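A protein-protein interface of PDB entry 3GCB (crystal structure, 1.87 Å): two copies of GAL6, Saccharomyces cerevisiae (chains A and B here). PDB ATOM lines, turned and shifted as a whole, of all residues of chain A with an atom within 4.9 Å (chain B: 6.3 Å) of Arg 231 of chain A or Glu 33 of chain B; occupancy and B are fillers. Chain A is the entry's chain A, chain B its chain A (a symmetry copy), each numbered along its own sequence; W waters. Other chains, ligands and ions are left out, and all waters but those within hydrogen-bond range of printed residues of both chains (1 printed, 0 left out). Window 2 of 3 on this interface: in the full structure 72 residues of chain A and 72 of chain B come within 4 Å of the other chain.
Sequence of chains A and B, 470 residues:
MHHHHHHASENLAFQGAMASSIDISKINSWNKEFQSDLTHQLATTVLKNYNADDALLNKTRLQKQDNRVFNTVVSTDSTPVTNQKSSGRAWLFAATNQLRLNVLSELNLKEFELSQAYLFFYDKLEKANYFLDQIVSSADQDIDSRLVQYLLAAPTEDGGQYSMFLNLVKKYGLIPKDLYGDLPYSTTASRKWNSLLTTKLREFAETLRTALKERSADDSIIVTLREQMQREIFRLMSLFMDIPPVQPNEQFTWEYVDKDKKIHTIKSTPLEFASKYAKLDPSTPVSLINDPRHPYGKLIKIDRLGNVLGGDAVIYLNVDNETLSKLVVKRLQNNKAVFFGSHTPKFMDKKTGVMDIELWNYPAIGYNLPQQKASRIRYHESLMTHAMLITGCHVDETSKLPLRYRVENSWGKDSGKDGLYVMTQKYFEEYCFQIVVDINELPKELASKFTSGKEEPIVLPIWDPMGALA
NH2 of Arg 231 of chain A lies within salt-bridge range of OE2 of Glu 33 of chain B, 2.7 Å away.
The guanidinium group (NH2) of Arg 235 of chain A lies within salt-bridge range of the side-chain carboxylate (OE2) of Glu 232 of chain A, 2.8 Å away.
The backbone carbonyl oxygen of Glu 33 of chain B lies within hydrogen-bond range of the side-chain hydroxyl of Ser 36 of chain B (2.6 Å).
Among the printed residues, merely in contact across the chains: Glu 227 of chain A with Trp 30 of chain B, Gln 230 of chain A with Trp 30 of chain B, Arg 231 of chain A with Trp 30 of chain B, Arg 231 of chain A with Phe 34 of chain B, Phe 234 of chain A with Asn 31 of chain B, Phe 234 of chain A with Phe 34 of chain B and Arg 235 of chain A with Phe 34 of chain B.
Arg 231 of chain A touches just these residues of chain B: Trp 30, Glu 33 and Phe 34.
Printed residues of chain A within 4 Å of Glu 33 of chain B: Arg 231 (2.7 Å).
Printed residues of chain B within 4 Å of Arg 235 of chain A: Phe 34.
Printed residues of chain B within 4 Å of Phe 234 of chain A: Asn 31 and Phe 34.
Printed residues of chain A within 4 Å of Trp 30 of chain B: Glu 227 (3.99 Å), Gln 230 (3.6 Å) and Arg 231 (3.6 Å).
Of the printed residues of chain B, Gln 230 of chain A touches Trp 30 (3.6 Å).
Ser 36 of chain B touches none of the printed residues of chain A.
Gln 35 of chain B touches none of the printed residues of chain A.
Hydrophobic or aromatic side chains of chain B within 4 Å of the printed part of chain A: Trp 30 and Phe 34.
Along chain B the printed residues that touch a printed residue of chain A span positions 30 to 34.
Of the 9 printed residues of chain A, 5 touch a printed residue of chain B.
Printed residues of chain A that touch a printed residue of chain B: Glu 227, Gln 230, Arg 231, Phe 234 and Arg 235.
Along chain A the printed residues that touch a printed residue of chain B span positions 227 to 235.
Among the printed residues, Asp or Glu carboxylates within 4 Å of a Lys or Arg side-chain nitrogen of the other chain: Arg 231 of chain A with Glu 33 of chain B (2.7 Å).
No position is printed for both chains.
Water W1 bridges NE1 of Trp 30 of chain B (2.9 Å) and OE2 of Glu 227 of chain A (3.4 Å).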
ATOM      1  N   GLU A 227      -7.117  -7.882 -11.899  1.00  0.00           N
ATOM      2  CA  GLU A 227      -7.033  -8.044 -10.456  1.00  0.00           C
ATOM      3  C   GLU A 227      -8.447  -8.135  -9.850  1.00  0.00           C
ATOM      4  O   GLU A 227      -8.735  -8.975  -8.990  1.00  0.00           O
ATOM      5  CB  GLU A 227      -6.278  -6.883  -9.825  1.00  0.00           C
ATOM      6  CG  GLU A 227      -5.997  -7.148  -8.357  1.00  0.00           C
ATOM      7  CD  GLU A 227      -5.262  -6.015  -7.676  1.00  0.00           C
ATOM      8  OE1 GLU A 227      -5.434  -4.853  -8.126  1.00  0.00           O
ATOM      9  OE2 GLU A 227      -4.534  -6.301  -6.699  1.00  0.00           O
ATOM     10  N   GLN A 228      -9.323  -7.256 -10.308  1.00  0.00           N
ATOM     11  CA  GLN A 228     -10.690  -7.255  -9.836  1.00  0.00           C
ATOM     12  C   GLN A 228     -11.389  -8.580 -10.202  1.00  0.00           C
ATOM     13  O   GLN A 228     -12.196  -9.085  -9.428  1.00  0.00           O
ATOM     14  CB  GLN A 228     -11.437  -6.068 -10.421  1.00  0.00           C
ATOM     15  CG  GLN A 228     -10.878  -4.715  -9.980  1.00  0.00           C
ATOM     16  CD  GLN A 228     -11.527  -3.533 -10.724  1.00  0.00           C
ATOM     17  OE1 GLN A 228     -12.251  -3.717 -11.717  1.00  0.00           O
ATOM     18  NE2 GLN A 228     -11.285  -2.318 -10.230  1.00  0.00           N
ATOM     19  N   MET A 229     -11.077  -9.132 -11.376  1.00  0.00           N
ATOM     20  CA  MET A 229     -11.662 -10.396 -11.817  1.00  0.00           C
ATOM     21  C   MET A 229     -11.156 -11.556 -10.973  1.00  0.00           C
ATOM     22  O   MET A 229     -11.928 -12.419 -10.573  1.00  0.00           O
ATOM     23  CB  MET A 229     -11.363 -10.609 -13.294  1.00  0.00           C
ATOM     24  CG  MET A 229     -12.124  -9.629 -14.127  1.00  0.00           C
ATOM     25  SD  MET A 229     -11.779  -9.751 -15.889  1.00  0.00           S
ATOM     26  CE  MET A 229     -13.032  -8.686 -16.525  1.00  0.00           C
ATOM     27  N   GLN A 230      -9.864 -11.556 -10.673  1.00  0.00           N
ATOM     28  CA  GLN A 230      -9.274 -12.595  -9.829  1.00  0.00           C
ATOM     29  C   GLN A 230      -9.976 -12.597  -8.469  1.00  0.00           C
ATOM     30  O   GLN A 230     -10.246 -13.648  -7.880  1.00  0.00           O
ATOM     31  CB  GLN A 230      -7.800 -12.294  -9.555  1.00  0.00           C
ATOM     32  CG  GLN A 230      -6.789 -12.874 -10.513  1.00  0.00           C
ATOM     33  CD  GLN A 230      -5.411 -12.911  -9.887  1.00  0.00           C
ATOM     34  OE1 GLN A 230      -5.220 -12.468  -8.738  1.00  0.00           O
ATOM     35  NE2 GLN A 230      -4.455 -13.455 -10.602  1.00  0.00           N
ATOM     36  N   ARG A 231     -10.192 -11.398  -7.943  1.00  0.00           N
ATOM     37  CA  ARG A 231     -10.805 -11.254  -6.630  1.00  0.00           C
ATOM     38  C   ARG A 231     -12.227 -11.797  -6.623  1.00  0.00           C
ATOM     39  O   ARG A 231     -12.644 -12.432  -5.653  1.00  0.00           O
ATOM     40  CB  ARG A 231     -10.787  -9.785  -6.206  1.00  0.00           C
ATOM     41  CG  ARG A 231     -11.380  -9.484  -4.818  1.00  0.00           C
ATOM     42  CD  ARG A 231     -11.254  -7.990  -4.554  1.00  0.00           C
ATOM     43  NE  ARG A 231     -11.691  -7.573  -3.224  1.00  0.00           N
ATOM     44  CZ  ARG A 231     -12.958  -7.370  -2.892  1.00  0.00           C
ATOM     45  NH1 ARG A 231     -13.925  -7.551  -3.783  1.00  0.00           N
ATOM     46  NH2 ARG A 231     -13.267  -6.954  -1.678  1.00  0.00           N
ATOM     47  N   GLU A 232     -12.975 -11.520  -7.689  1.00  0.00           N
ATOM     48  CA  GLU A 232     -14.337 -11.986  -7.782  1.00  0.00           C
ATOM     49  C   GLU A 232     -14.365 -13.500  -7.949  1.00  0.00           C
ATOM     50  O   GLU A 232     -15.212 -14.172  -7.369  1.00  0.00           O
ATOM     51  CB  GLU A 232     -15.068 -11.278  -8.925  1.00  0.00           C
ATOM     52  CG  GLU A 232     -16.548 -11.683  -9.115  1.00  0.00           C
ATOM     53  CD  GLU A 232     -17.447 -11.471  -7.879  1.00  0.00           C
ATOM     54  OE1 GLU A 232     -17.035 -10.822  -6.882  1.00  0.00           O
ATOM     55  OE2 GLU A 232     -18.593 -11.971  -7.922  1.00  0.00           O
ATOM     56  N   ILE A 233     -13.419 -14.036  -8.713  1.00  0.00           N
ATOM     57  CA  ILE A 233     -13.341 -15.488  -8.893  1.00  0.00           C
ATOM     58  C   ILE A 233     -13.051 -16.139  -7.544  1.00  0.00           C
ATOM     59  O   ILE A 233     -13.700 -17.127  -7.177  1.00  0.00           O
ATOM     60  CB  ILE A 233     -12.232 -15.888  -9.884  1.00  0.00           C
ATOM     61  CG1 ILE A 233     -12.612 -15.448 -11.303  1.00  0.00           C
ATOM     62  CG2 ILE A 233     -12.011 -17.404  -9.854  1.00  0.00           C
ATOM     63  CD1 ILE A 233     -11.411 -15.499 -12.240  1.00  0.00           C
ATOM     64  N   PHE A 234     -12.081 -15.589  -6.806  1.00  0.00           N
ATOM     65  CA  PHE A 234     -11.746 -16.146  -5.497  1.00  0.00           C
ATOM     66  C   PHE A 234     -12.951 -16.026  -4.566  1.00  0.00           C
ATOM     67  O   PHE A 234     -13.260 -16.972  -3.825  1.00  0.00           O
ATOM     68  CB  PHE A 234     -10.519 -15.476  -4.836  1.00  0.00           C
ATOM     69  CG  PHE A 234     -10.230 -16.027  -3.463  1.00  0.00           C
ATOM     70  CD1 PHE A 234      -9.648 -17.291  -3.317  1.00  0.00           C
ATOM     71  CD2 PHE A 234     -10.689 -15.372  -2.327  1.00  0.00           C
ATOM     72  CE1 PHE A 234      -9.547 -17.894  -2.050  1.00  0.00           C
ATOM     73  CE2 PHE A 234     -10.591 -15.960  -1.072  1.00  0.00           C
ATOM     74  CZ  PHE A 234     -10.025 -17.217  -0.934  1.00  0.00           C
ATOM     75  N   ARG A 235     -13.635 -14.881  -4.620  1.00  0.00           N
ATOM     76  CA  ARG A 235     -14.800 -14.651  -3.761  1.00  0.00           C
ATOM     77  C   ARG A 235     -15.846 -15.745  -3.963  1.00  0.00           C
ATOM     78  O   ARG A 235     -16.355 -16.309  -2.989  1.00  0.00           O
ATOM     79  CB  ARG A 235     -15.445 -13.279  -4.022  1.00  0.00           C
ATOM     80  CG  ARG A 235     -16.474 -12.920  -2.949  1.00  0.00           C
ATOM     81  CD  ARG A 235     -17.254 -11.684  -3.308  1.00  0.00           C
ATOM     82  NE  ARG A 235     -18.099 -11.888  -4.484  1.00  0.00           N
ATOM     83  CZ  ARG A 235     -19.361 -12.308  -4.459  1.00  0.00           C
ATOM     84  NH1 ARG A 235     -19.959 -12.592  -3.315  1.00  0.00           N
ATOM     85  NH2 ARG A 235     -20.054 -12.370  -5.582  1.00  0.00           N
ATOM     86  N   ASN B  28      -5.233 -15.122   0.500  1.00  0.00           N
ATOM     87  CA  ASN B  28      -5.474 -15.310   1.931  1.00  0.00           C
ATOM     88  C   ASN B  28      -5.895 -13.995   2.576  1.00  0.00           C
ATOM     89  O   ASN B  28      -6.691 -13.982   3.527  1.00  0.00           O
ATOM     90  CB  ASN B  28      -4.264 -15.916   2.621  1.00  0.00           C
ATOM     91  CG  ASN B  28      -4.245 -17.421   2.506  1.00  0.00           C
ATOM     92  OD1 ASN B  28      -4.857 -18.139   3.304  1.00  0.00           O
ATOM     93  ND2 ASN B  28      -3.551 -17.913   1.494  1.00  0.00           N
ATOM     94  N   SER B  29      -5.415 -12.884   2.019  1.00  0.00           N
ATOM     95  CA  SER B  29      -5.789 -11.560   2.500  1.00  0.00           C
ATOM     96  C   SER B  29      -7.246 -11.282   2.076  1.00  0.00           C
ATOM     97  O   SER B  29      -8.052 -10.792   2.875  1.00  0.00           O
ATOM     98  CB  SER B  29      -4.839 -10.517   1.926  1.00  0.00           C
ATOM     99  OG  SER B  29      -3.527 -10.763   2.410  1.00  0.00           O
ATOM    100  N   TRP B  30      -7.600 -11.624   0.835  1.00  0.00           N
ATOM    101  CA  TRP B  30      -8.974 -11.440   0.396  1.00  0.00           C
ATOM    102  C   TRP B  30      -9.886 -12.331   1.262  1.00  0.00           C
ATOM    103  O   TRP B  30     -10.989 -11.931   1.620  1.00  0.00           O
ATOM    104  CB  TRP B  30      -9.145 -11.849  -1.055  1.00  0.00           C
ATOM    105  CG  TRP B  30      -8.631 -10.880  -2.055  1.00  0.00           C
ATOM    106  CD1 TRP B  30      -8.547  -9.513  -1.935  1.00  0.00           C
ATOM    107  CD2 TRP B  30      -8.154 -11.191  -3.377  1.00  0.00           C
ATOM    108  NE1 TRP B  30      -8.060  -8.961  -3.104  1.00  0.00           N
ATOM    109  CE2 TRP B  30      -7.823  -9.968  -4.005  1.00  0.00           C
ATOM    110  CE3 TRP B  30      -8.003 -12.396  -4.089  1.00  0.00           C
ATOM    111  CZ2 TRP B  30      -7.321  -9.910  -5.318  1.00  0.00           C
ATOM    112  CZ3 TRP B  30      -7.503 -12.343  -5.393  1.00  0.00           C
ATOM    113  CH2 TRP B  30      -7.181 -11.110  -5.999  1.00  0.00           C
ATOM    114  N   ASN B  31      -9.427 -13.530   1.604  1.00  0.00           N
ATOM    115  CA  ASN B  31     -10.244 -14.421   2.422  1.00  0.00           C
ATOM    116  C   ASN B  31     -10.583 -13.779   3.791  1.00  0.00           C
ATOM    117  O   ASN B  31     -11.727 -13.822   4.272  1.00  0.00           O
ATOM    118  CB  ASN B  31      -9.535 -15.758   2.614  1.00  0.00           C
ATOM    119  CG  ASN B  31     -10.438 -16.813   3.242  1.00  0.00           C
ATOM    120  OD1 ASN B  31     -11.486 -17.149   2.696  1.00  0.00           O
ATOM    121  ND2 ASN B  31     -10.041 -17.324   4.399  1.00  0.00           N
ATOM    122  N   LYS B  32      -9.573 -13.184   4.412  1.00  0.00           N
ATOM    123  CA  LYS B  32      -9.764 -12.527   5.703  1.00  0.00           C
ATOM    124  C   LYS B  32     -10.828 -11.416   5.587  1.00  0.00           C
ATOM    125  O   LYS B  32     -11.724 -11.302   6.433  1.00  0.00           O
ATOM    126  CB  LYS B  32      -8.429 -11.951   6.170  1.00  0.00           C
ATOM    127  CG  LYS B  32      -8.415 -11.568   7.618  1.00  0.00           C
ATOM    128  CD  LYS B  32      -7.075 -10.923   8.010  1.00  0.00           C
ATOM    129  CE  LYS B  32      -7.134 -10.423   9.466  1.00  0.00           C
ATOM    130  NZ  LYS B  32      -6.239  -9.244   9.704  1.00  0.00           N
ATOM    131  N   GLU B  33     -10.757 -10.625   4.518  1.00  0.00           N
ATOM    132  CA  GLU B  33     -11.718  -9.542   4.311  1.00  0.00           C
ATOM    133  C   GLU B  33     -13.135 -10.079   4.083  1.00  0.00           C
ATOM    134  O   GLU B  33     -14.112  -9.535   4.617  1.00  0.00           O
ATOM    135  CB  GLU B  33     -11.302  -8.699   3.115  1.00  0.00           C
ATOM    136  CG  GLU B  33     -12.309  -7.635   2.687  1.00  0.00           C
ATOM    137  CD  GLU B  33     -11.891  -6.936   1.387  1.00  0.00           C
ATOM    138  OE1 GLU B  33     -10.783  -7.236   0.868  1.00  0.00           O
ATOM    139  OE2 GLU B  33     -12.665  -6.108   0.863  1.00  0.00           O
ATOM    140  N   PHE B  34     -13.257 -11.114   3.249  1.00  0.00           N
ATOM    141  CA  PHE B  34     -14.566 -11.700   2.971  1.00  0.00           C
ATOM    142  C   PHE B  34     -15.186 -12.293   4.223  1.00  0.00           C
ATOM    143  O   PHE B  34     -16.376 -12.097   4.475  1.00  0.00           O
ATOM    144  CB  PHE B  34     -14.468 -12.747   1.863  1.00  0.00           C
ATOM    145  CG  PHE B  34     -14.121 -12.162   0.505  1.00  0.00           C
ATOM    146  CD1 PHE B  34     -14.580 -10.903   0.139  1.00  0.00           C
ATOM    147  CD2 PHE B  34     -13.317 -12.859  -0.388  1.00  0.00           C
ATOM    148  CE1 PHE B  34     -14.238 -10.353  -1.083  1.00  0.00           C
ATOM    149  CE2 PHE B  34     -12.978 -12.307  -1.598  1.00  0.00           C
ATOM    150  CZ  PHE B  34     -13.435 -11.054  -1.948  1.00  0.00           C
ATOM    151  N   GLN B  35     -14.373 -12.954   5.039  1.00  0.00           N
ATOM    152  CA  GLN B  35     -14.884 -13.548   6.272  1.00  0.00           C
ATOM    153  C   GLN B  35     -15.373 -12.511   7.305  1.00  0.00           C
ATOM    154  O   GLN B  35     -16.129 -12.849   8.213  1.00  0.00           O
ATOM    155  CB  GLN B  35     -13.854 -14.504   6.886  1.00  0.00           C
ATOM    156  CG  GLN B  35     -13.586 -15.764   6.068  1.00  0.00           C
ATOM    157  CD  GLN B  35     -14.832 -16.643   5.863  1.00  0.00           C
ATOM    158  OE1 GLN B  35     -15.723 -16.716   6.724  1.00  0.00           O
ATOM    159  NE2 GLN B  35     -14.883 -17.335   4.723  1.00  0.00           N
ATOM    160  N   SER B  36     -15.000 -11.242   7.131  1.00  0.00           N
ATOM    161  CA  SER B  36     -15.445 -10.181   8.043  1.00  0.00           C
ATOM    162  C   SER B  36     -16.873  -9.755   7.690  1.00  0.00           C
ATOM    163  O   SER B  36     -17.532  -9.045   8.443  1.00  0.00           O
ATOM    164  CB  SER B  36     -14.513  -8.965   7.967  1.00  0.00           C
ATOM    165  OG  SER B  36     -14.732  -8.183   6.790  1.00  0.00           O
ATOM    166  N   ASP B  37     -17.317 -10.162   6.510  1.00  0.00           N
ATOM    167  CA  ASP B  37     -18.650  -9.828   6.037  1.00  0.00           C
ATOM    168  C   ASP B  37     -19.640 -10.931   6.445  1.00  0.00           C
ATOM    169  O   ASP B  37     -19.470 -12.101   6.089  1.00  0.00           O
ATOM    170  CB  ASP B  37     -18.601  -9.652   4.524  1.00  0.00           C
ATOM    171  CG  ASP B  37     -19.920  -9.216   3.948  1.00  0.00           C
ATOM    172  OD1 ASP B  37     -20.339  -8.067   4.191  1.00  0.00           O
ATOM    173  OD2 ASP B  37     -20.555 -10.019   3.249  1.00  0.00           O
HETATM  174  O   HOH W   1      -6.887  -6.622  -4.325  1.00  0.00           O
